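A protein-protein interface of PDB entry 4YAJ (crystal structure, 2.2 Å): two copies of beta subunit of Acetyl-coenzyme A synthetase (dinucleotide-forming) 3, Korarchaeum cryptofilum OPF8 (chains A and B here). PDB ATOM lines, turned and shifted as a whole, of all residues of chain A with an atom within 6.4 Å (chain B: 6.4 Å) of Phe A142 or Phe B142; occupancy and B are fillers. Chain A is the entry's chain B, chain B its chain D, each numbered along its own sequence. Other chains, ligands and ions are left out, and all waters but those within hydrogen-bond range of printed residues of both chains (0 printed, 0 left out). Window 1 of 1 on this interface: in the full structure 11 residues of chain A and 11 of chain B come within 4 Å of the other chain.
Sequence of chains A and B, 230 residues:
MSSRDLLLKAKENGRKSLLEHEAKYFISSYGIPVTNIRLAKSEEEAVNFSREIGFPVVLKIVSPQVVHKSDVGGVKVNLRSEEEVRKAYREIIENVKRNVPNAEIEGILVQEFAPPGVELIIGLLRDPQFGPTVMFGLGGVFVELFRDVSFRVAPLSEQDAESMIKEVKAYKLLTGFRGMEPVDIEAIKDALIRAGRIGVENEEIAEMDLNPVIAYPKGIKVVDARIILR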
ATOM      1  N   GLY A 137      -0.639   8.930 -28.541  1.00  0.00           N
ATOM      2  CA  GLY A 137       0.439   9.004 -27.573  1.00  0.00           C
ATOM      3  C   GLY A 137       1.600   8.108 -27.950  1.00  0.00           C
ATOM      4  O   GLY A 137       1.474   7.252 -28.824  1.00  0.00           O
ATOM      5  N   LEU A 138       2.736   8.311 -27.291  1.00  0.00           N
ATOM      6  CA  LEU A 138       3.894   7.448 -27.483  1.00  0.00           C
ATOM      7  C   LEU A 138       3.739   6.209 -26.611  1.00  0.00           C
ATOM      8  O   LEU A 138       3.123   6.260 -25.544  1.00  0.00           O
ATOM      9  CB  LEU A 138       5.188   8.188 -27.136  1.00  0.00           C
ATOM     10  CG  LEU A 138       5.764   9.169 -28.164  1.00  0.00           C
ATOM     11  CD1 LEU A 138       6.439   8.420 -29.298  1.00  0.00           C
ATOM     12  CD2 LEU A 138       4.697  10.108 -28.711  1.00  0.00           C
ATOM     13  N   GLY A 139       4.306   5.097 -27.063  1.00  0.00           N
ATOM     14  CA  GLY A 139       4.109   3.827 -26.393  1.00  0.00           C
ATOM     15  C   GLY A 139       4.950   3.673 -25.143  1.00  0.00           C
ATOM     16  O   GLY A 139       5.596   4.619 -24.690  1.00  0.00           O
ATOM     17  N   GLY A 140       4.954   2.459 -24.604  1.00  0.00           N
ATOM     18  CA  GLY A 140       5.687   2.158 -23.392  1.00  0.00           C
ATOM     19  C   GLY A 140       5.190   2.929 -22.186  1.00  0.00           C
ATOM     20  O   GLY A 140       3.984   3.040 -21.947  1.00  0.00           O
ATOM     21  N   VAL A 141       6.136   3.469 -21.426  1.00  0.00           N
ATOM     22  CA  VAL A 141       5.822   4.148 -20.179  1.00  0.00           C
ATOM     23  C   VAL A 141       5.044   5.434 -20.418  1.00  0.00           C
ATOM     24  O   VAL A 141       4.261   5.856 -19.568  1.00  0.00           O
ATOM     25  CB  VAL A 141       7.103   4.485 -19.384  1.00  0.00           C
ATOM     26  CG1 VAL A 141       7.818   3.211 -18.970  1.00  0.00           C
ATOM     27  CG2 VAL A 141       8.036   5.377 -20.202  1.00  0.00           C
ATOM     28  N   PHE A 142       5.231   6.028 -21.591  1.00  0.00           N
ATOM     29  CA  PHE A 142       4.739   7.377 -21.841  1.00  0.00           C
ATOM     30  C   PHE A 142       3.219   7.457 -21.771  1.00  0.00           C
ATOM     31  O   PHE A 142       2.677   8.444 -21.277  1.00  0.00           O
ATOM     32  CB  PHE A 142       5.253   7.876 -23.187  1.00  0.00           C
ATOM     33  CG  PHE A 142       6.746   8.007 -23.236  1.00  0.00           C
ATOM     34  CD1 PHE A 142       7.371   9.118 -22.700  1.00  0.00           C
ATOM     35  CD2 PHE A 142       7.525   7.009 -23.791  1.00  0.00           C
ATOM     36  CE1 PHE A 142       8.744   9.237 -22.730  1.00  0.00           C
ATOM     37  CE2 PHE A 142       8.899   7.124 -23.824  1.00  0.00           C
ATOM     38  CZ  PHE A 142       9.509   8.240 -23.291  1.00  0.00           C
ATOM     39  N   VAL A 143       2.535   6.418 -22.236  1.00  0.00           N
ATOM     40  CA  VAL A 143       1.092   6.320 -22.035  1.00  0.00           C
ATOM     41  C   VAL A 143       0.791   5.539 -20.760  1.00  0.00           C
ATOM     42  O   VAL A 143       0.027   6.003 -19.911  1.00  0.00           O
ATOM     43  CB  VAL A 143       0.389   5.655 -23.241  1.00  0.00           C
ATOM     44  CG1 VAL A 143      -0.971   5.071 -22.846  1.00  0.00           C
ATOM     45  CG2 VAL A 143       0.210   6.657 -24.361  1.00  0.00           C
ATOM     46  N   GLU A 144       1.400   4.365 -20.623  1.00  0.00           N
ATOM     47  CA  GLU A 144       1.067   3.456 -19.528  1.00  0.00           C
ATOM     48  C   GLU A 144       1.311   4.066 -18.154  1.00  0.00           C
ATOM     49  O   GLU A 144       0.546   3.828 -17.222  1.00  0.00           O
ATOM     50  CB  GLU A 144       1.869   2.158 -19.648  1.00  0.00           C
ATOM     51  CG  GLU A 144       1.435   1.253 -20.787  1.00  0.00           C
ATOM     52  CD  GLU A 144       2.260  -0.016 -20.863  1.00  0.00           C
ATOM     53  OE1 GLU A 144       3.107  -0.231 -19.969  1.00  0.00           O
ATOM     54  OE2 GLU A 144       2.064  -0.800 -21.815  1.00  0.00           O
ATOM     55  N   LEU A 145       2.371   4.860 -18.037  1.00  0.00           N
ATOM     56  CA  LEU A 145       2.801   5.377 -16.744  1.00  0.00           C
ATOM     57  C   LEU A 145       2.559   6.875 -16.609  1.00  0.00           C
ATOM     58  O   LEU A 145       2.022   7.328 -15.599  1.00  0.00           O
ATOM     59  CB  LEU A 145       4.286   5.069 -16.528  1.00  0.00           C
ATOM     60  CG  LEU A 145       4.873   5.398 -15.155  1.00  0.00           C
ATOM     61  CD1 LEU A 145       4.167   4.623 -14.051  1.00  0.00           C
ATOM     62  CD2 LEU A 145       6.364   5.109 -15.143  1.00  0.00           C
ATOM     63  N   PHE A 146       2.946   7.642 -17.622  1.00  0.00           N
ATOM     64  CA  PHE A 146       2.842   9.096 -17.550  1.00  0.00           C
ATOM     65  C   PHE A 146       1.510   9.619 -18.089  1.00  0.00           C
ATOM     66  O   PHE A 146       1.179  10.786 -17.889  1.00  0.00           O
ATOM     67  CB  PHE A 146       4.000   9.745 -18.310  1.00  0.00           C
ATOM     68  CG  PHE A 146       5.352   9.390 -17.765  1.00  0.00           C
ATOM     69  CD1 PHE A 146       5.666   9.634 -16.440  1.00  0.00           C
ATOM     70  CD2 PHE A 146       6.315   8.822 -18.581  1.00  0.00           C
ATOM     71  CE1 PHE A 146       6.910   9.308 -15.936  1.00  0.00           C
ATOM     72  CE2 PHE A 146       7.560   8.496 -18.083  1.00  0.00           C
ATOM     73  CZ  PHE A 146       7.858   8.741 -16.759  1.00  0.00           C
ATOM     74  N   ARG A 147       0.752   8.756 -18.761  1.00  0.00           N
ATOM     75  CA  ARG A 147      -0.545   9.134 -19.325  1.00  0.00           C
ATOM     76  C   ARG A 147      -0.441  10.343 -20.258  1.00  0.00           C
ATOM     77  O   ARG A 147      -1.363  11.142 -20.376  1.00  0.00           O
ATOM     78  CB  ARG A 147      -1.544   9.422 -18.197  1.00  0.00           C
ATOM     79  CG  ARG A 147      -1.994   8.180 -17.450  1.00  0.00           C
ATOM     80  CD  ARG A 147      -2.665   8.527 -16.130  1.00  0.00           C
ATOM     81  NE  ARG A 147      -3.643   7.517 -15.733  1.00  0.00           N
ATOM     82  CZ  ARG A 147      -3.338   6.353 -15.165  1.00  0.00           C
ATOM     83  NH1 ARG A 147      -4.305   5.505 -14.842  1.00  0.00           N
ATOM     84  NH2 ARG A 147      -2.074   6.032 -14.921  1.00  0.00           N
ATOM     85  N   ASP A 148       0.673  10.447 -20.968  1.00  0.00           N
ATOM     86  CA  ASP A 148       0.880  11.552 -21.898  1.00  0.00           C
ATOM     87  C   ASP A 148       0.123  11.339 -23.208  1.00  0.00           C
ATOM     88  O   ASP A 148       0.669  10.755 -24.141  1.00  0.00           O
ATOM     89  CB  ASP A 148       2.371  11.725 -22.187  1.00  0.00           C
ATOM     90  CG  ASP A 148       2.654  12.879 -23.129  1.00  0.00           C
ATOM     91  OD1 ASP A 148       1.916  13.884 -23.077  1.00  0.00           O
ATOM     92  OD2 ASP A 148       3.614  12.779 -23.921  1.00  0.00           O
ATOM     93  N   VAL A 149      -1.115  11.827 -23.277  1.00  0.00           N
ATOM     94  CA  VAL A 149      -1.980  11.582 -24.434  1.00  0.00           C
ATOM     95  C   VAL A 149      -2.659  12.860 -24.910  1.00  0.00           C
ATOM     96  O   VAL A 149      -2.848  13.797 -24.134  1.00  0.00           O
ATOM     97  CB  VAL A 149      -3.070  10.533 -24.119  1.00  0.00           C
ATOM     98  CG1 VAL A 149      -2.438   9.198 -23.777  1.00  0.00           C
ATOM     99  CG2 VAL A 149      -3.974  11.010 -22.989  1.00  0.00           C
ATOM    100  N   ALA A 170       6.009  14.010 -25.158  1.00  0.00           N
ATOM    101  CA  ALA A 170       7.046  13.122 -25.668  1.00  0.00           C
ATOM    102  C   ALA A 170       7.213  13.273 -27.177  1.00  0.00           C
ATOM    103  O   ALA A 170       7.687  12.352 -27.849  1.00  0.00           O
ATOM    104  CB  ALA A 170       6.720  11.680 -25.316  1.00  0.00           C
ATOM    105  N   LEU A 173      10.451  12.478 -29.421  1.00  0.00           N
ATOM    106  CA  LEU A 173      10.832  11.112 -29.767  1.00  0.00           C
ATOM    107  C   LEU A 173      10.526  10.765 -31.225  1.00  0.00           C
ATOM    108  O   LEU A 173      10.949   9.722 -31.717  1.00  0.00           O
ATOM    109  CB  LEU A 173      10.122  10.115 -28.849  1.00  0.00           C
ATOM    110  CG  LEU A 173      10.681   9.930 -27.437  1.00  0.00           C
ATOM    111  CD1 LEU A 173       9.838   8.930 -26.675  1.00  0.00           C
ATOM    112  CD2 LEU A 173      12.136   9.484 -27.447  1.00  0.00           C
ATOM    113  N   GLY B 137      18.479  14.038 -12.553  1.00  0.00           N
ATOM    114  CA  GLY B 137      17.528  13.626 -13.568  1.00  0.00           C
ATOM    115  C   GLY B 137      17.690  12.161 -13.923  1.00  0.00           C
ATOM    116  O   GLY B 137      18.696  11.541 -13.583  1.00  0.00           O
ATOM    117  N   LEU B 138      16.693  11.605 -14.604  1.00  0.00           N
ATOM    118  CA  LEU B 138      16.774  10.241 -15.115  1.00  0.00           C
ATOM    119  C   LEU B 138      17.478  10.213 -16.468  1.00  0.00           C
ATOM    120  O   LEU B 138      17.493  11.210 -17.199  1.00  0.00           O
ATOM    121  CB  LEU B 138      15.385   9.614 -15.218  1.00  0.00           C
ATOM    122  CG  LEU B 138      14.848   9.103 -13.879  1.00  0.00           C
ATOM    123  CD1 LEU B 138      14.017  10.161 -13.174  1.00  0.00           C
ATOM    124  CD2 LEU B 138      14.052   7.831 -14.078  1.00  0.00           C
ATOM    125  N   GLY B 139      18.094   9.075 -16.773  1.00  0.00           N
ATOM    126  CA  GLY B 139      18.929   8.953 -17.950  1.00  0.00           C
ATOM    127  C   GLY B 139      18.226   8.775 -19.273  1.00  0.00           C
ATOM    128  O   GLY B 139      17.005   8.896 -19.379  1.00  0.00           O
ATOM    129  N   GLY B 140      19.028   8.470 -20.285  1.00  0.00           N
ATOM    130  CA  GLY B 140      18.542   8.325 -21.637  1.00  0.00           C
ATOM    131  C   GLY B 140      17.971   9.629 -22.145  1.00  0.00           C
ATOM    132  O   GLY B 140      18.550  10.704 -21.958  1.00  0.00           O
ATOM    133  N   VAL B 141      16.811   9.530 -22.777  1.00  0.00           N
ATOM    134  CA  VAL B 141      16.185  10.677 -23.407  1.00  0.00           C
ATOM    135  C   VAL B 141      15.723  11.706 -22.383  1.00  0.00           C
ATOM    136  O   VAL B 141      15.675  12.897 -22.680  1.00  0.00           O
ATOM    137  CB  VAL B 141      14.978  10.245 -24.264  1.00  0.00           C
ATOM    138  CG1 VAL B 141      15.440   9.373 -25.419  1.00  0.00           C
ATOM    139  CG2 VAL B 141      13.944   9.510 -23.414  1.00  0.00           C
ATOM    140  N   PHE B 142      15.435  11.256 -21.165  1.00  0.00           N
ATOM    141  CA  PHE B 142      14.739  12.105 -20.205  1.00  0.00           C
ATOM    142  C   PHE B 142      15.533  13.350 -19.828  1.00  0.00           C
ATOM    143  O   PHE B 142      14.951  14.421 -19.667  1.00  0.00           O
ATOM    144  CB  PHE B 142      14.382  11.299 -18.956  1.00  0.00           C
ATOM    145  CG  PHE B 142      13.418  10.183 -19.226  1.00  0.00           C
ATOM    146  CD1 PHE B 142      12.061  10.434 -19.323  1.00  0.00           C
ATOM    147  CD2 PHE B 142      13.867   8.888 -19.406  1.00  0.00           C
ATOM    148  CE1 PHE B 142      11.173   9.411 -19.581  1.00  0.00           C
ATOM    149  CE2 PHE B 142      12.984   7.864 -19.663  1.00  0.00           C
ATOM    150  CZ  PHE B 142      11.634   8.125 -19.753  1.00  0.00           C
ATOM    151  N   VAL B 143      16.851  13.225 -19.713  1.00  0.00           N
ATOM    152  CA  VAL B 143      17.697  14.404 -19.550  1.00  0.00           C
ATOM    153  C   VAL B 143      18.204  14.874 -20.909  1.00  0.00           C
ATOM    154  O   VAL B 143      18.092  16.055 -21.251  1.00  0.00           O
ATOM    155  CB  VAL B 143      18.903  14.142 -18.603  1.00  0.00           C
ATOM    156  CG1 VAL B 143      19.679  12.892 -19.007  1.00  0.00           C
ATOM    157  CG2 VAL B 143      19.835  15.355 -18.561  1.00  0.00           C
ATOM    158  N   GLU B 144      18.750  13.942 -21.681  1.00  0.00           N
ATOM    159  CA  GLU B 144      19.440  14.269 -22.921  1.00  0.00           C
ATOM    160  C   GLU B 144      18.530  14.965 -23.928  1.00  0.00           C
ATOM    161  O   GLU B 144      18.970  15.857 -24.652  1.00  0.00           O
ATOM    162  CB  GLU B 144      20.031  13.000 -23.536  1.00  0.00           C
ATOM    163  CG  GLU B 144      21.067  13.259 -24.614  1.00  0.00           C
ATOM    164  CD  GLU B 144      21.822  12.006 -25.009  1.00  0.00           C
ATOM    165  OE1 GLU B 144      21.557  10.937 -24.418  1.00  0.00           O
ATOM    166  OE2 GLU B 144      22.685  12.088 -25.907  1.00  0.00           O
ATOM    167  N   LEU B 145      17.263  14.559 -23.960  1.00  0.00           N
ATOM    168  CA  LEU B 145      16.327  15.033 -24.975  1.00  0.00           C
ATOM    169  C   LEU B 145      15.254  15.954 -24.399  1.00  0.00           C
ATOM    170  O   LEU B 145      14.980  17.014 -24.958  1.00  0.00           O
ATOM    171  CB  LEU B 145      15.666  13.841 -25.670  1.00  0.00           C
ATOM    172  CG  LEU B 145      14.784  14.149 -26.879  1.00  0.00           C
ATOM    173  CD1 LEU B 145      15.577  14.821 -27.990  1.00  0.00           C
ATOM    174  CD2 LEU B 145      14.133  12.872 -27.374  1.00  0.00           C
ATOM    175  N   PHE B 146      14.646  15.549 -23.288  1.00  0.00           N
ATOM    176  CA  PHE B 146      13.544  16.311 -22.703  1.00  0.00           C
ATOM    177  C   PHE B 146      14.014  17.344 -21.683  1.00  0.00           C
ATOM    178  O   PHE B 146      13.235  18.200 -21.265  1.00  0.00           O
ATOM    179  CB  PHE B 146      12.537  15.372 -22.037  1.00  0.00           C
ATOM    180  CG  PHE B 146      11.887  14.404 -22.982  1.00  0.00           C
ATOM    181  CD1 PHE B 146      11.199  14.856 -24.094  1.00  0.00           C
ATOM    182  CD2 PHE B 146      11.951  13.044 -22.748  1.00  0.00           C
ATOM    183  CE1 PHE B 146      10.598  13.967 -24.960  1.00  0.00           C
ATOM    184  CE2 PHE B 146      11.350  12.149 -23.609  1.00  0.00           C
ATOM    185  CZ  PHE B 146      10.671  12.613 -24.716  1.00  0.00           C
ATOM    186  N   ARG B 147      15.281  17.264 -21.284  1.00  0.00           N
ATOM    187  CA  ARG B 147      15.840  18.191 -20.303  1.00  0.00           C
ATOM    188  C   ARG B 147      15.038  18.195 -19.003  1.00  0.00           C
ATOM    189  O   ARG B 147      14.936  19.210 -18.322  1.00  0.00           O
ATOM    190  CB  ARG B 147      15.896  19.607 -20.881  1.00  0.00           C
ATOM    191  N   ASP B 148      14.505  17.036 -18.631  1.00  0.00           N
ATOM    192  CA  ASP B 148      13.737  16.915 -17.399  1.00  0.00           C
ATOM    193  C   ASP B 148      14.689  16.869 -16.210  1.00  0.00           C
ATOM    194  O   ASP B 148      15.108  15.792 -15.792  1.00  0.00           O
ATOM    195  CB  ASP B 148      12.862  15.662 -17.433  1.00  0.00           C
ATOM    196  CG  ASP B 148      12.032  15.495 -16.178  1.00  0.00           C
ATOM    197  OD1 ASP B 148      11.623  16.517 -15.589  1.00  0.00           O
ATOM    198  OD2 ASP B 148      11.790  14.339 -15.778  1.00  0.00           O
ATOM    199  N   VAL B 149      15.003  18.039 -15.661  1.00  0.00           N
ATOM    200  CA  VAL B 149      16.039  18.158 -14.642  1.00  0.00           C
ATOM    201  C   VAL B 149      15.605  19.015 -13.457  1.00  0.00           C
ATOM    202  O   VAL B 149      14.768  19.907 -13.598  1.00  0.00           O
ATOM    203  CB  VAL B 149      17.324  18.749 -15.275  1.00  0.00           C
ATOM    204  CG1 VAL B 149      18.239  19.365 -14.238  1.00  0.00           C
ATOM    205  CG2 VAL B 149      18.053  17.684 -16.073  1.00  0.00           C
ATOM    206  N   ALA B 170       9.812  12.613 -14.640  1.00  0.00           N
ATOM    207  CA  ALA B 170      10.041  11.187 -14.827  1.00  0.00           C
ATOM    208  C   ALA B 170      10.266  10.494 -13.489  1.00  0.00           C
ATOM    209  O   ALA B 170      10.864   9.418 -13.431  1.00  0.00           O
ATOM    210  CB  ALA B 170      11.227  10.960 -15.749  1.00  0.00           C
ATOM    211  N   LEU B 173       9.371   6.707 -12.618  1.00  0.00           N
ATOM    212  CA  LEU B 173      10.251   5.623 -13.055  1.00  0.00           C
ATOM    213  C   LEU B 173      11.085   5.038 -11.912  1.00  0.00           C
ATOM    214  O   LEU B 173      11.774   4.037 -12.096  1.00  0.00           O
ATOM    215  CB  LEU B 173      11.179   6.111 -14.169  1.00  0.00           C
ATOM    216  CG  LEU B 173      10.604   6.207 -15.585  1.00  0.00           C
ATOM    217  CD1 LEU B 173      11.650   6.744 -16.545  1.00  0.00           C
ATOM    218  CD2 LEU B 173      10.094   4.862 -16.083  1.00  0.00           C
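The backbone carbonyl oxygen of Phe A142 lies within hydrogen-bond range of the backbone NH of Arg A147, 3.2 Å away. O of Val B141 sits at hydrogen-bond distance from N of Phe B146, 2.9 Å away. The backbone NH of Ala B170 is in hydrogen-bond range of the side-chain carboxylate of Asp B148 (2.9 Å). The side-chain carboxylate (OD2) of Asp A148 sits at hydrogen-bond distance from the backbone NH (N) of Ala A170. N of Arg B147 lies within hydrogen-bond range of O of Phe B142. O of Phe B142 is in hydrogen-bond range of N of Asp B148 (2.8 Å).
Among the printed residues, merely in contact across the chains: Phe A142 with Phe B142 (3.98 Å), Leu A145 with Leu B173 (3.9 Å), Phe A146 with Ala B170 (3.8 Å), Phe A146 with Leu B173 (3.9 Å), Ala A170 with Phe B146 (3.7 Å), Leu A173 with Val B141 (3.9 Å), Leu A173 with Leu B145 (3.9 Å) and Leu A173 with Phe B146 (3.8 Å).
Printed residues of chain B within 4 Å of Phe A142: Phe B142. Of the printed residues of chain A, Phe B142 touches Phe A142 (3.98 Å). Of the printed residues of chain A, Val B141 touches Leu A173 (3.9 Å). Printed residues of chain B within 4 Å of Ala A170: Phe B146 (3.7 Å). Gly A139 touches none of the printed residues of chain B. Asp A148 touches none of the printed residues of chain B. The nearest printed residue of chain B that does not touch Phe A142 is Phe B146 (4.01 Å).
Hydrophobic or aromatic side chains of chain B within 4 Å of the printed part of chain A: Val B141, Phe B142, Leu B145, Phe B146 and Leu B173. Of the 15 printed residues of chain A, 5 touch a printed residue of chain B. Hydrophobic or aromatic side chains of chain A within 4 Å of the printed part of chain B: Phe A142, Leu A145, Phe A146 and Leu A173.
Leu A145 touches Leu B173, and with the chains exchanged Leu A173 touches Leu B145. Phe A146 touches Ala B170, and with the chains exchanged Ala A170 touches Phe B146. Phe A146 touches Leu B173, and with the chains exchanged Leu A173 touches Phe B146. Leu A173 touches Val B141, but with the chains exchanged Val A141 does not touch Leu B173 (4.03 Å). Positions printed for both chains: 137, 138, 139, 140, 141, 142, 143, 144, 145, 146, 147, 148, 149, 170 and 173. Of the 8 pairs that touch across the chains among the printed residues, 7 have their exchanged pair printed and touching as well.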
